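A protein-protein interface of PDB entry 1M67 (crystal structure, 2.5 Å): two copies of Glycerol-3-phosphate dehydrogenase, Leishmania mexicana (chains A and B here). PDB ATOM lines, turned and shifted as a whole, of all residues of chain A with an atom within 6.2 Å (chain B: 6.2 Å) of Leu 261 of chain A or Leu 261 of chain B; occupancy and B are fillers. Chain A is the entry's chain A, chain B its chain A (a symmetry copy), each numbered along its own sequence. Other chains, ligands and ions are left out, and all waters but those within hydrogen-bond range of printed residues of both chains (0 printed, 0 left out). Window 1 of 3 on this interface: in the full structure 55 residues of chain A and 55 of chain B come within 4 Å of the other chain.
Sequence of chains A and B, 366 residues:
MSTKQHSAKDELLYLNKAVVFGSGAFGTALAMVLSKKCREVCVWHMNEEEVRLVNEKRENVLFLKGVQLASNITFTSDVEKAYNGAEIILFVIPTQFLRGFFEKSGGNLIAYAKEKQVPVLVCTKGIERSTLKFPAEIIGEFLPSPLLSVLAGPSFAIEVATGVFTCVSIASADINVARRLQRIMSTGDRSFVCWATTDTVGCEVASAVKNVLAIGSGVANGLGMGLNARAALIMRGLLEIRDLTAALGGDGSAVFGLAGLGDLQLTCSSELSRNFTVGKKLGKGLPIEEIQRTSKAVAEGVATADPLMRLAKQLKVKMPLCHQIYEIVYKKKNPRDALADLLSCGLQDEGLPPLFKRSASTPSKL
Of the printed residues of chain B, Ile 234 of chain A touches Gln 265 (3.6 Å).
Printed residues of chain B within 4 Å of Leu 238 of chain A: Leu 261 (3.8 Å).
Of chain B, only Leu 238 (3.8 Å) and Leu 261 (3.0 Å) come within 4 Å of Leu 261 of chain A.
Leu 261 of chain B touches just these residues of chain A: Leu 238 (3.8 Å) and Leu 261 (3.0 Å).
Leu 264 of chain B touches none of the printed residues of chain A.
The nearest printed residue of chain B that does not touch Leu 261 of chain A is Ile 234 of chain B (4.4 Å).
The nearest printed residue of chain A that does not touch Leu 261 of chain B is Ile 234 of chain A (4.4 Å).
The nearest printed residue of chain A that does not touch Ala 231 of chain B is Leu 266 of chain A (4.3 Å).
The side-chain sulfur (SD) of Met 235 of chain A lies within hydrogen-bond range of the backbone NH (N) of Leu 258 of chain B (3.6 Å).
N of Leu 258 of chain A is in hydrogen-bond range of SD of Met 235 of chain B (3.6 Å).
The side-chain amide oxygen (OE1) of Gln 265 of chain A lies close to the side-chain amide oxygen (OE1) of Gln 265 of chain B, at 2.8 Å.
Of the 19 printed residues of chain A, 11 touch a printed residue of chain B.
Printed residues of chain A that touch a printed residue of chain B: Pro 154, Ala 231, Ile 234, Met 235, Leu 238, Phe 256, Gly 257, Leu 258, Leu 261, Gly 262 and Gln 265.
Along chain A the printed residues that touch a printed residue of chain B span positions 154 to 265.
Among the printed residues, no Asp or Glu carboxylate lies within 4 Å of a Lys or Arg side-chain nitrogen of the other chain.
The backbone NH (N) of Leu 261 of chain A sits at hydrogen-bond distance from the backbone carbonyl oxygen (O) of Val 255 of chain A (3.0 Å).
The backbone carbonyl oxygen of Gly 257 of chain A lies within hydrogen-bond range of the backbone NH of Gly 262 of chain A, 3.0 Å away.
The backbone carbonyl oxygen (O) of Leu 258 of chain A sits at hydrogen-bond distance from the backbone NH (N) of Asp 263 of chain A (2.9 Å).
The backbone carbonyl oxygen (O) of Val 255 of chain B sits at hydrogen-bond distance from the backbone NH (N) of Leu 261 of chain B, 3.0 Å away.
The backbone NH (N) of Gly 262 of chain B is in hydrogen-bond range of the backbone carbonyl oxygen (O) of Gly 257 of chain B, 3.0 Å away.
The backbone carbonyl oxygen (O) of Leu 258 of chain B is in hydrogen-bond range of the backbone NH (N) of Asp 263 of chain B, at 2.9 Å.
Pro 154 of chain A touches Ala 231 of chain B, and with the chains exchanged Ala 231 of chain A touches Pro 154 of chain B.
Ala 231 of chain A touches Gly 262 of chain B, and with the chains exchanged Gly 262 of chain A touches Ala 231 of chain B.
Ala 231 of chain A touches Gln 265 of chain B, and with the chains exchanged Gln 265 of chain A touches Ala 231 of chain B.
Leu 261 of chain B touches its own counterpart, Leu 261 of chain A.
Positions printed for both chains: 154, 206, 231, 234, 235, 238, 254, 255, 256, 257, 258, 259, 260, 261, 262, 263, 264, 265 and 266.
Of the 19 pairs that touch across the chains among the printed residues, 19 have their exchanged pair printed and touching as well.
Among the printed residues, pairs that only touch across the chains: Pro 154 of chain A with Ala 231 of chain B, Ala 231 of chain A with Pro 154 of chain B, Ala 231 of chain A with Gly 262 of chain B, Ala 231 of chain A with Gln 265 of chain B, Ile 234 of chain A with Gln 265 of chain B, Met 235 of chain A with Phe 256 of chain B, Met 235 of chain A with Gly 257 of chain B, Leu 238 of chain A with Leu 261 of chain B, Phe 256 of chain A with Met 235 of chain B, Phe 256 of chain A with Phe 256 of chain B, Gly 257 of chain A with Met 235 of chain B, Leu 261 of chain A with Leu 238 of chain B, Leu 261 of chain A with Leu 261 of chain B, Gly 262 of chain A with Ala 231 of chain B, Gln 265 of chain A with Ala 231 of chain B and Gln 265 of chain A with Ile 234 of chain B.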
ATOM      1  N   PRO A 154      35.948   0.977 -13.650  1.00  0.00           N
ATOM      2  CA  PRO A 154      36.646   1.425 -12.443  1.00  0.00           C
ATOM      3  C   PRO A 154      38.127   1.312 -12.719  1.00  0.00           C
ATOM      4  O   PRO A 154      38.609   0.191 -12.850  1.00  0.00           O
ATOM      5  CB  PRO A 154      36.235   0.402 -11.387  1.00  0.00           C
ATOM      6  CG  PRO A 154      35.275  -0.540 -12.059  1.00  0.00           C
ATOM      7  CD  PRO A 154      35.444  -0.399 -13.538  1.00  0.00           C
ATOM      8  N   ALA A 206      27.234   7.540 -17.205  1.00  0.00           N
ATOM      9  CA  ALA A 206      27.927   7.093 -15.963  1.00  0.00           C
ATOM     10  C   ALA A 206      29.246   7.840 -15.720  1.00  0.00           C
ATOM     11  O   ALA A 206      29.496   8.321 -14.627  1.00  0.00           O
ATOM     12  CB  ALA A 206      28.165   5.584 -15.951  1.00  0.00           C
ATOM     13  N   ALA A 231      27.045   4.005   0.818  1.00  0.00           N
ATOM     14  CA  ALA A 231      26.464   2.891   0.071  1.00  0.00           C
ATOM     15  C   ALA A 231      25.106   3.266  -0.488  1.00  0.00           C
ATOM     16  O   ALA A 231      24.815   2.972  -1.639  1.00  0.00           O
ATOM     17  CB  ALA A 231      26.343   1.664   0.949  1.00  0.00           C
ATOM     18  N   ILE A 234      25.464   5.661  -3.471  1.00  0.00           N
ATOM     19  CA  ILE A 234      25.854   4.957  -4.688  1.00  0.00           C
ATOM     20  C   ILE A 234      24.672   4.279  -5.360  1.00  0.00           C
ATOM     21  O   ILE A 234      24.530   4.331  -6.569  1.00  0.00           O
ATOM     22  CB  ILE A 234      26.938   3.922  -4.357  1.00  0.00           C
ATOM     23  CG1 ILE A 234      28.273   4.640  -4.114  1.00  0.00           C
ATOM     24  CG2 ILE A 234      27.055   2.911  -5.473  1.00  0.00           C
ATOM     25  CD1 ILE A 234      29.255   3.884  -3.210  1.00  0.00           C
ATOM     26  N   MET A 235      23.825   3.650  -4.556  1.00  0.00           N
ATOM     27  CA  MET A 235      22.658   2.925  -5.046  1.00  0.00           C
ATOM     28  C   MET A 235      21.590   3.851  -5.630  1.00  0.00           C
ATOM     29  O   MET A 235      21.128   3.620  -6.742  1.00  0.00           O
ATOM     30  CB  MET A 235      22.098   2.034  -3.925  1.00  0.00           C
ATOM     31  CG  MET A 235      21.053   1.000  -4.342  1.00  0.00           C
ATOM     32  SD  MET A 235      19.302   1.553  -4.170  1.00  0.00           S
ATOM     33  CE  MET A 235      18.825   1.718  -5.889  1.00  0.00           C
ATOM     34  N   LEU A 238      22.854   5.807  -8.752  1.00  0.00           N
ATOM     35  CA  LEU A 238      22.806   5.002  -9.975  1.00  0.00           C
ATOM     36  C   LEU A 238      21.482   5.116 -10.742  1.00  0.00           C
ATOM     37  O   LEU A 238      21.484   5.118 -11.972  1.00  0.00           O
ATOM     38  CB  LEU A 238      23.128   3.540  -9.663  1.00  0.00           C
ATOM     39  CG  LEU A 238      23.764   2.707 -10.778  1.00  0.00           C
ATOM     40  CD1 LEU A 238      25.134   3.221 -11.189  1.00  0.00           C
ATOM     41  CD2 LEU A 238      23.833   1.245 -10.375  1.00  0.00           C
ATOM     42  N   ALA A 254      24.992  -0.714 -19.798  1.00  0.00           N
ATOM     43  CA  ALA A 254      26.258  -0.403 -19.138  1.00  0.00           C
ATOM     44  C   ALA A 254      26.043   0.065 -17.715  1.00  0.00           C
ATOM     45  O   ALA A 254      26.980   0.058 -16.902  1.00  0.00           O
ATOM     46  CB  ALA A 254      27.003   0.647 -19.890  1.00  0.00           C
ATOM     47  N   VAL A 255      24.808   0.447 -17.417  1.00  0.00           N
ATOM     48  CA  VAL A 255      24.444   1.028 -16.130  1.00  0.00           C
ATOM     49  C   VAL A 255      24.780   0.190 -14.906  1.00  0.00           C
ATOM     50  O   VAL A 255      25.374   0.687 -13.949  1.00  0.00           O
ATOM     51  CB  VAL A 255      22.928   1.396 -16.087  1.00  0.00           C
ATOM     52  CG1 VAL A 255      22.543   1.903 -14.714  1.00  0.00           C
ATOM     53  CG2 VAL A 255      22.615   2.423 -17.165  1.00  0.00           C
ATOM     54  N   PHE A 256      24.368  -1.067 -14.900  1.00  0.00           N
ATOM     55  CA  PHE A 256      24.667  -1.896 -13.752  1.00  0.00           C
ATOM     56  C   PHE A 256      25.937  -2.678 -13.932  1.00  0.00           C
ATOM     57  O   PHE A 256      26.176  -3.593 -13.193  1.00  0.00           O
ATOM     58  CB  PHE A 256      23.505  -2.796 -13.375  1.00  0.00           C
ATOM     59  CG  PHE A 256      22.317  -2.042 -12.885  1.00  0.00           C
ATOM     60  CD1 PHE A 256      21.109  -2.095 -13.567  1.00  0.00           C
ATOM     61  CD2 PHE A 256      22.416  -1.254 -11.750  1.00  0.00           C
ATOM     62  CE1 PHE A 256      20.017  -1.386 -13.115  1.00  0.00           C
ATOM     63  CE2 PHE A 256      21.327  -0.547 -11.295  1.00  0.00           C
ATOM     64  CZ  PHE A 256      20.127  -0.607 -11.973  1.00  0.00           C
ATOM     65  N   GLY A 257      26.775  -2.258 -14.875  1.00  0.00           N
ATOM     66  CA  GLY A 257      28.036  -2.926 -15.135  1.00  0.00           C
ATOM     67  C   GLY A 257      29.281  -2.144 -14.752  1.00  0.00           C
ATOM     68  O   GLY A 257      29.248  -1.283 -13.861  1.00  0.00           O
ATOM     69  N   LEU A 258      30.379  -2.424 -15.440  1.00  0.00           N
ATOM     70  CA  LEU A 258      31.651  -1.811 -15.095  1.00  0.00           C
ATOM     71  C   LEU A 258      31.659  -0.291 -15.195  1.00  0.00           C
ATOM     72  O   LEU A 258      32.185   0.387 -14.308  1.00  0.00           O
ATOM     73  CB  LEU A 258      32.777  -2.409 -15.929  1.00  0.00           C
ATOM     74  CG  LEU A 258      33.176  -3.824 -15.479  1.00  0.00           C
ATOM     75  CD1 LEU A 258      34.013  -4.539 -16.546  1.00  0.00           C
ATOM     76  CD2 LEU A 258      33.879  -3.796 -14.130  1.00  0.00           C
ATOM     77  N   ALA A 259      31.057   0.229 -16.268  1.00  0.00           N
ATOM     78  CA  ALA A 259      31.042   1.664 -16.543  1.00  0.00           C
ATOM     79  C   ALA A 259      30.155   2.396 -15.568  1.00  0.00           C
ATOM     80  O   ALA A 259      30.432   3.549 -15.194  1.00  0.00           O
ATOM     81  CB  ALA A 259      30.586   1.921 -17.951  1.00  0.00           C
ATOM     82  N   GLY A 260      29.093   1.720 -15.140  1.00  0.00           N
ATOM     83  CA  GLY A 260      28.161   2.299 -14.188  1.00  0.00           C
ATOM     84  C   GLY A 260      28.465   1.984 -12.736  1.00  0.00           C
ATOM     85  O   GLY A 260      29.256   2.657 -12.114  1.00  0.00           O
ATOM     86  N   LEU A 261      27.825   0.963 -12.182  1.00  0.00           N
ATOM     87  CA  LEU A 261      28.036   0.617 -10.778  1.00  0.00           C
ATOM     88  C   LEU A 261      29.509   0.526 -10.411  1.00  0.00           C
ATOM     89  O   LEU A 261      29.915   1.033  -9.372  1.00  0.00           O
ATOM     90  CB  LEU A 261      27.343  -0.710 -10.426  1.00  0.00           C
ATOM     91  CG  LEU A 261      27.924  -1.510  -9.240  1.00  0.00           C
ATOM     92  CD1 LEU A 261      28.166  -0.677  -7.959  1.00  0.00           C
ATOM     93  CD2 LEU A 261      27.051  -2.724  -8.936  1.00  0.00           C
ATOM     94  N   GLY A 262      30.292  -0.125 -11.267  1.00  0.00           N
ATOM     95  CA  GLY A 262      31.703  -0.332 -11.032  1.00  0.00           C
ATOM     96  C   GLY A 262      32.480   0.954 -10.849  1.00  0.00           C
ATOM     97  O   GLY A 262      33.116   1.150  -9.812  1.00  0.00           O
ATOM     98  N   ASP A 263      32.420   1.845 -11.836  1.00  0.00           N
ATOM     99  CA  ASP A 263      33.184   3.083 -11.759  1.00  0.00           C
ATOM    100  C   ASP A 263      32.594   3.996 -10.693  1.00  0.00           C
ATOM    101  O   ASP A 263      33.309   4.760 -10.040  1.00  0.00           O
ATOM    102  CB  ASP A 263      33.220   3.781 -13.120  1.00  0.00           C
ATOM    103  CG  ASP A 263      34.371   4.768 -13.245  1.00  0.00           C
ATOM    104  OD1 ASP A 263      34.593   5.312 -14.350  1.00  0.00           O
ATOM    105  OD2 ASP A 263      35.125   5.052 -12.302  1.00  0.00           O
ATOM    106  N   LEU A 264      31.285   3.879 -10.492  1.00  0.00           N
ATOM    107  CA  LEU A 264      30.599   4.734  -9.537  1.00  0.00           C
ATOM    108  C   LEU A 264      31.016   4.401  -8.117  1.00  0.00           C
ATOM    109  O   LEU A 264      31.330   5.292  -7.326  1.00  0.00           O
ATOM    110  CB  LEU A 264      29.079   4.611  -9.685  1.00  0.00           C
ATOM    111  CG  LEU A 264      28.316   5.471  -8.672  1.00  0.00           C
ATOM    112  CD1 LEU A 264      28.696   6.916  -8.828  1.00  0.00           C
ATOM    113  CD2 LEU A 264      26.807   5.298  -8.811  1.00  0.00           C
ATOM    114  N   GLN A 265      31.019   3.111  -7.793  1.00  0.00           N
ATOM    115  CA  GLN A 265      31.371   2.702  -6.446  1.00  0.00           C
ATOM    116  C   GLN A 265      32.814   3.126  -6.177  1.00  0.00           C
ATOM    117  O   GLN A 265      33.112   3.736  -5.158  1.00  0.00           O
ATOM    118  CB  GLN A 265      31.123   1.201  -6.252  1.00  0.00           C
ATOM    119  CG  GLN A 265      32.318   0.311  -6.481  1.00  0.00           C
ATOM    120  CD  GLN A 265      33.110   0.090  -5.224  1.00  0.00           C
ATOM    121  OE1 GLN A 265      32.551   0.045  -4.130  1.00  0.00           O
ATOM    122  NE2 GLN A 265      34.411  -0.056  -5.374  1.00  0.00           N
ATOM    123  N   LEU A 266      33.699   2.862  -7.130  1.00  0.00           N
ATOM    124  CA  LEU A 266      35.088   3.264  -6.986  1.00  0.00           C
ATOM    125  C   LEU A 266      35.262   4.760  -6.718  1.00  0.00           C
ATOM    126  O   LEU A 266      35.828   5.170  -5.699  1.00  0.00           O
ATOM    127  CB  LEU A 266      35.878   2.904  -8.241  1.00  0.00           C
ATOM    128  CG  LEU A 266      37.383   3.164  -8.130  1.00  0.00           C
ATOM    129  CD1 LEU A 266      38.003   2.118  -7.219  1.00  0.00           C
ATOM    130  CD2 LEU A 266      38.060   3.164  -9.486  1.00  0.00           C
ATOM    131  N   PRO B 154      22.573  -1.830   3.356  1.00  0.00           N
ATOM    132  CA  PRO B 154      23.917  -1.567   3.873  1.00  0.00           C
ATOM    133  C   PRO B 154      23.755  -0.996   5.262  1.00  0.00           C
ATOM    134  O   PRO B 154      23.253   0.118   5.376  1.00  0.00           O
ATOM    135  CB  PRO B 154      24.465  -0.497   2.932  1.00  0.00           C
ATOM    136  CG  PRO B 154      23.401  -0.259   1.896  1.00  0.00           C
ATOM    137  CD  PRO B 154      22.108  -0.791   2.427  1.00  0.00           C
ATOM    138  N   ALA B 206      20.994 -11.970  -1.775  1.00  0.00           N
ATOM    139  CA  ALA B 206      22.032 -10.922  -1.556  1.00  0.00           C
ATOM    140  C   ALA B 206      22.659 -10.992  -0.157  1.00  0.00           C
ATOM    141  O   ALA B 206      23.870 -10.966  -0.017  1.00  0.00           O
ATOM    142  CB  ALA B 206      21.492  -9.518  -1.822  1.00  0.00           C
ATOM    143  N   ALA B 231      36.231  -3.204  -7.099  1.00  0.00           N
ATOM    144  CA  ALA B 231      35.068  -2.697  -7.823  1.00  0.00           C
ATOM    145  C   ALA B 231      34.573  -3.717  -8.829  1.00  0.00           C
ATOM    146  O   ALA B 231      33.375  -3.939  -8.934  1.00  0.00           O
ATOM    147  CB  ALA B 231      35.400  -1.397  -8.524  1.00  0.00           C
ATOM    148  N   ILE B 234      32.766  -6.615  -7.068  1.00  0.00           N
ATOM    149  CA  ILE B 234      31.415  -6.245  -6.663  1.00  0.00           C
ATOM    150  C   ILE B 234      30.431  -6.320  -7.818  1.00  0.00           C
ATOM    151  O   ILE B 234      29.324  -6.805  -7.663  1.00  0.00           O
ATOM    152  CB  ILE B 234      31.425  -4.829  -6.069  1.00  0.00           C
ATOM    153  CG1 ILE B 234      32.043  -4.869  -4.664  1.00  0.00           C
ATOM    154  CG2 ILE B 234      30.025  -4.265  -6.037  1.00  0.00           C
ATOM    155  CD1 ILE B 234      32.678  -3.550  -4.205  1.00  0.00           C
ATOM    156  N   MET B 235      30.855  -5.838  -8.979  1.00  0.00           N
ATOM    157  CA  MET B 235      30.023  -5.808 -10.176  1.00  0.00           C
ATOM    158  C   MET B 235      29.739  -7.204 -10.733  1.00  0.00           C
ATOM    159  O   MET B 235      28.585  -7.534 -10.985  1.00  0.00           O
ATOM    160  CB  MET B 235      30.665  -4.887 -11.227  1.00  0.00           C
ATOM    161  CG  MET B 235      29.795  -4.519 -12.427  1.00  0.00           C
ATOM    162  SD  MET B 235      30.003  -5.609 -13.900  1.00  0.00           S
ATOM    163  CE  MET B 235      28.439  -6.484 -13.904  1.00  0.00           C
ATOM    164  N   LEU B 238      27.721  -9.422  -8.247  1.00  0.00           N
ATOM    165  CA  LEU B 238      26.285  -9.132  -8.276  1.00  0.00           C
ATOM    166  C   LEU B 238      25.501  -9.978  -9.287  1.00  0.00           C
ATOM    167  O   LEU B 238      24.370 -10.374  -9.010  1.00  0.00           O
ATOM    168  CB  LEU B 238      26.048  -7.641  -8.517  1.00  0.00           C
ATOM    169  CG  LEU B 238      24.763  -7.034  -7.950  1.00  0.00           C
ATOM    170  CD1 LEU B 238      24.705  -7.091  -6.432  1.00  0.00           C
ATOM    171  CD2 LEU B 238      24.585  -5.610  -8.444  1.00  0.00           C
ATOM    172  N   ALA B 254      15.272  -6.484  -5.902  1.00  0.00           N
ATOM    173  CA  ALA B 254      16.113  -6.064  -4.784  1.00  0.00           C
ATOM    174  C   ALA B 254      17.581  -6.096  -5.150  1.00  0.00           C
ATOM    175  O   ALA B 254      18.412  -5.474  -4.471  1.00  0.00           O
ATOM    176  CB  ALA B 254      15.887  -6.933  -3.595  1.00  0.00           C
ATOM    177  N   VAL B 255      17.888  -6.800  -6.231  1.00  0.00           N
ATOM    178  CA  VAL B 255      19.260  -7.031  -6.668  1.00  0.00           C
ATOM    179  C   VAL B 255      20.100  -5.785  -6.899  1.00  0.00           C
ATOM    180  O   VAL B 255      21.224  -5.684  -6.406  1.00  0.00           O
ATOM    181  CB  VAL B 255      19.302  -7.912  -7.955  1.00  0.00           C
ATOM    182  CG1 VAL B 255      20.722  -8.058  -8.454  1.00  0.00           C
ATOM    183  CG2 VAL B 255      18.669  -9.267  -7.674  1.00  0.00           C
ATOM    184  N   PHE B 256      19.591  -4.847  -7.683  1.00  0.00           N
ATOM    185  CA  PHE B 256      20.360  -3.647  -7.928  1.00  0.00           C
ATOM    186  C   PHE B 256      20.014  -2.544  -6.969  1.00  0.00           C
ATOM    187  O   PHE B 256      20.370  -1.423  -7.206  1.00  0.00           O
ATOM    188  CB  PHE B 256      20.261  -3.185  -9.370  1.00  0.00           C
ATOM    189  CG  PHE B 256      20.890  -4.133 -10.332  1.00  0.00           C
ATOM    190  CD1 PHE B 256      20.132  -4.764 -11.309  1.00  0.00           C
ATOM    191  CD2 PHE B 256      22.242  -4.417 -10.241  1.00  0.00           C
ATOM    192  CE1 PHE B 256      20.717  -5.649 -12.189  1.00  0.00           C
ATOM    193  CE2 PHE B 256      22.831  -5.298 -11.119  1.00  0.00           C
ATOM    194  CZ  PHE B 256      22.074  -5.918 -12.093  1.00  0.00           C
ATOM    195  N   GLY B 257      19.382  -2.892  -5.853  1.00  0.00           N
ATOM    196  CA  GLY B 257      19.004  -1.918  -4.847  1.00  0.00           C
ATOM    197  C   GLY B 257      19.767  -2.001  -3.536  1.00  0.00           C
ATOM    198  O   GLY B 257      20.911  -2.476  -3.489  1.00  0.00           O
ATOM    199  N   LEU B 258      19.127  -1.562  -2.461  1.00  0.00           N
ATOM    200  CA  LEU B 258      19.793  -1.502  -1.171  1.00  0.00           C
ATOM    201  C   LEU B 258      20.278  -2.850  -0.655  1.00  0.00           C
ATOM    202  O   LEU B 258      21.400  -2.956  -0.151  1.00  0.00           O
ATOM    203  CB  LEU B 258      18.901  -0.822  -0.140  1.00  0.00           C
ATOM    204  CG  LEU B 258      18.815   0.702  -0.325  1.00  0.00           C
ATOM    205  CD1 LEU B 258      17.637   1.298   0.454  1.00  0.00           C
ATOM    206  CD2 LEU B 258      20.132   1.376   0.030  1.00  0.00           C
ATOM    207  N   ALA B 259      19.432  -3.873  -0.803  1.00  0.00           N
ATOM    208  CA  ALA B 259      19.723  -5.212  -0.296  1.00  0.00           C
ATOM    209  C   ALA B 259      20.817  -5.873  -1.096  1.00  0.00           C
ATOM    210  O   ALA B 259      21.624  -6.649  -0.556  1.00  0.00           O
ATOM    211  CB  ALA B 259      18.482  -6.059  -0.320  1.00  0.00           C
ATOM    212  N   GLY B 260      20.857  -5.552  -2.386  1.00  0.00           N
ATOM    213  CA  GLY B 260      21.869  -6.103  -3.271  1.00  0.00           C
ATOM    214  C   GLY B 260      23.114  -5.249  -3.416  1.00  0.00           C
ATOM    215  O   GLY B 260      24.014  -5.334  -2.611  1.00  0.00           O
ATOM    216  N   LEU B 261      23.179  -4.429  -4.456  1.00  0.00           N
ATOM    217  CA  LEU B 261      24.359  -3.598  -4.685  1.00  0.00           C
ATOM    218  C   LEU B 261      24.798  -2.844  -3.440  1.00  0.00           C
ATOM    219  O   LEU B 261      25.983  -2.797  -3.135  1.00  0.00           O
ATOM    220  CB  LEU B 261      24.117  -2.597  -5.827  1.00  0.00           C
ATOM    221  CG  LEU B 261      24.959  -1.302  -5.812  1.00  0.00           C
ATOM    222  CD1 LEU B 261      26.477  -1.524  -5.608  1.00  0.00           C
ATOM    223  CD2 LEU B 261      24.698  -0.482  -7.072  1.00  0.00           C
ATOM    224  N   GLY B 262      23.833  -2.256  -2.736  1.00  0.00           N
ATOM    225  CA  GLY B 262      24.100  -1.465  -1.555  1.00  0.00           C
ATOM    226  C   GLY B 262      24.827  -2.228  -0.469  1.00  0.00           C
ATOM    227  O   GLY B 262      25.914  -1.826  -0.052  1.00  0.00           O
ATOM    228  N   ASP B 263      24.251  -3.340  -0.019  1.00  0.00           N
ATOM    229  CA  ASP B 263      24.861  -4.101   1.063  1.00  0.00           C
ATOM    230  C   ASP B 263      26.135  -4.776   0.575  1.00  0.00           C
ATOM    231  O   ASP B 263      27.091  -4.959   1.331  1.00  0.00           O
ATOM    232  CB  ASP B 263      23.875  -5.129   1.623  1.00  0.00           C
ATOM    233  CG  ASP B 263      24.240  -5.589   3.027  1.00  0.00           C
ATOM    234  OD1 ASP B 263      23.448  -6.331   3.652  1.00  0.00           O
ATOM    235  OD2 ASP B 263      25.284  -5.248   3.602  1.00  0.00           O
ATOM    236  N   LEU B 264      26.157  -5.107  -0.712  1.00  0.00           N
ATOM    237  CA  LEU B 264      27.297  -5.804  -1.284  1.00  0.00           C
ATOM    238  C   LEU B 264      28.516  -4.902  -1.323  1.00  0.00           C
ATOM    239  O   LEU B 264      29.612  -5.303  -0.925  1.00  0.00           O
ATOM    240  CB  LEU B 264      26.976  -6.321  -2.690  1.00  0.00           C
ATOM    241  CG  LEU B 264      28.165  -7.033  -3.343  1.00  0.00           C
ATOM    242  CD1 LEU B 264      28.605  -8.193  -2.495  1.00  0.00           C
ATOM    243  CD2 LEU B 264      27.834  -7.499  -4.757  1.00  0.00           C
ATOM    244  N   GLN B 265      28.325  -3.677  -1.806  1.00  0.00           N
ATOM    245  CA  GLN B 265      29.443  -2.758  -1.912  1.00  0.00           C
ATOM    246  C   GLN B 265      29.983  -2.492  -0.509  1.00  0.00           C
ATOM    247  O   GLN B 265      31.179  -2.582  -0.266  1.00  0.00           O
ATOM    248  CB  GLN B 265      29.030  -1.487  -2.665  1.00  0.00           C
ATOM    249  CG  GLN B 265      28.590  -0.334  -1.799  1.00  0.00           C
ATOM    250  CD  GLN B 265      29.735   0.561  -1.420  1.00  0.00           C
ATOM    251  OE1 GLN B 265      30.675   0.738  -2.193  1.00  0.00           O
ATOM    252  NE2 GLN B 265      29.661   1.133  -0.235  1.00  0.00           N
ATOM    253  N   LEU B 266      29.086  -2.233   0.434  1.00  0.00           N
ATOM    254  CA  LEU B 266      29.498  -2.008   1.810  1.00  0.00           C
ATOM    255  C   LEU B 266      30.327  -3.155   2.390  1.00  0.00           C
ATOM    256  O   LEU B 266      31.473  -2.970   2.815  1.00  0.00           O
ATOM    257  CB  LEU B 266      28.277  -1.798   2.703  1.00  0.00           C
ATOM    258  CG  LEU B 266      28.615  -1.417   4.146  1.00  0.00           C
ATOM    259  CD1 LEU B 266      29.114   0.018   4.180  1.00  0.00           C
ATOM    260  CD2 LEU B 266      27.428  -1.595   5.072  1.00  0.00           C
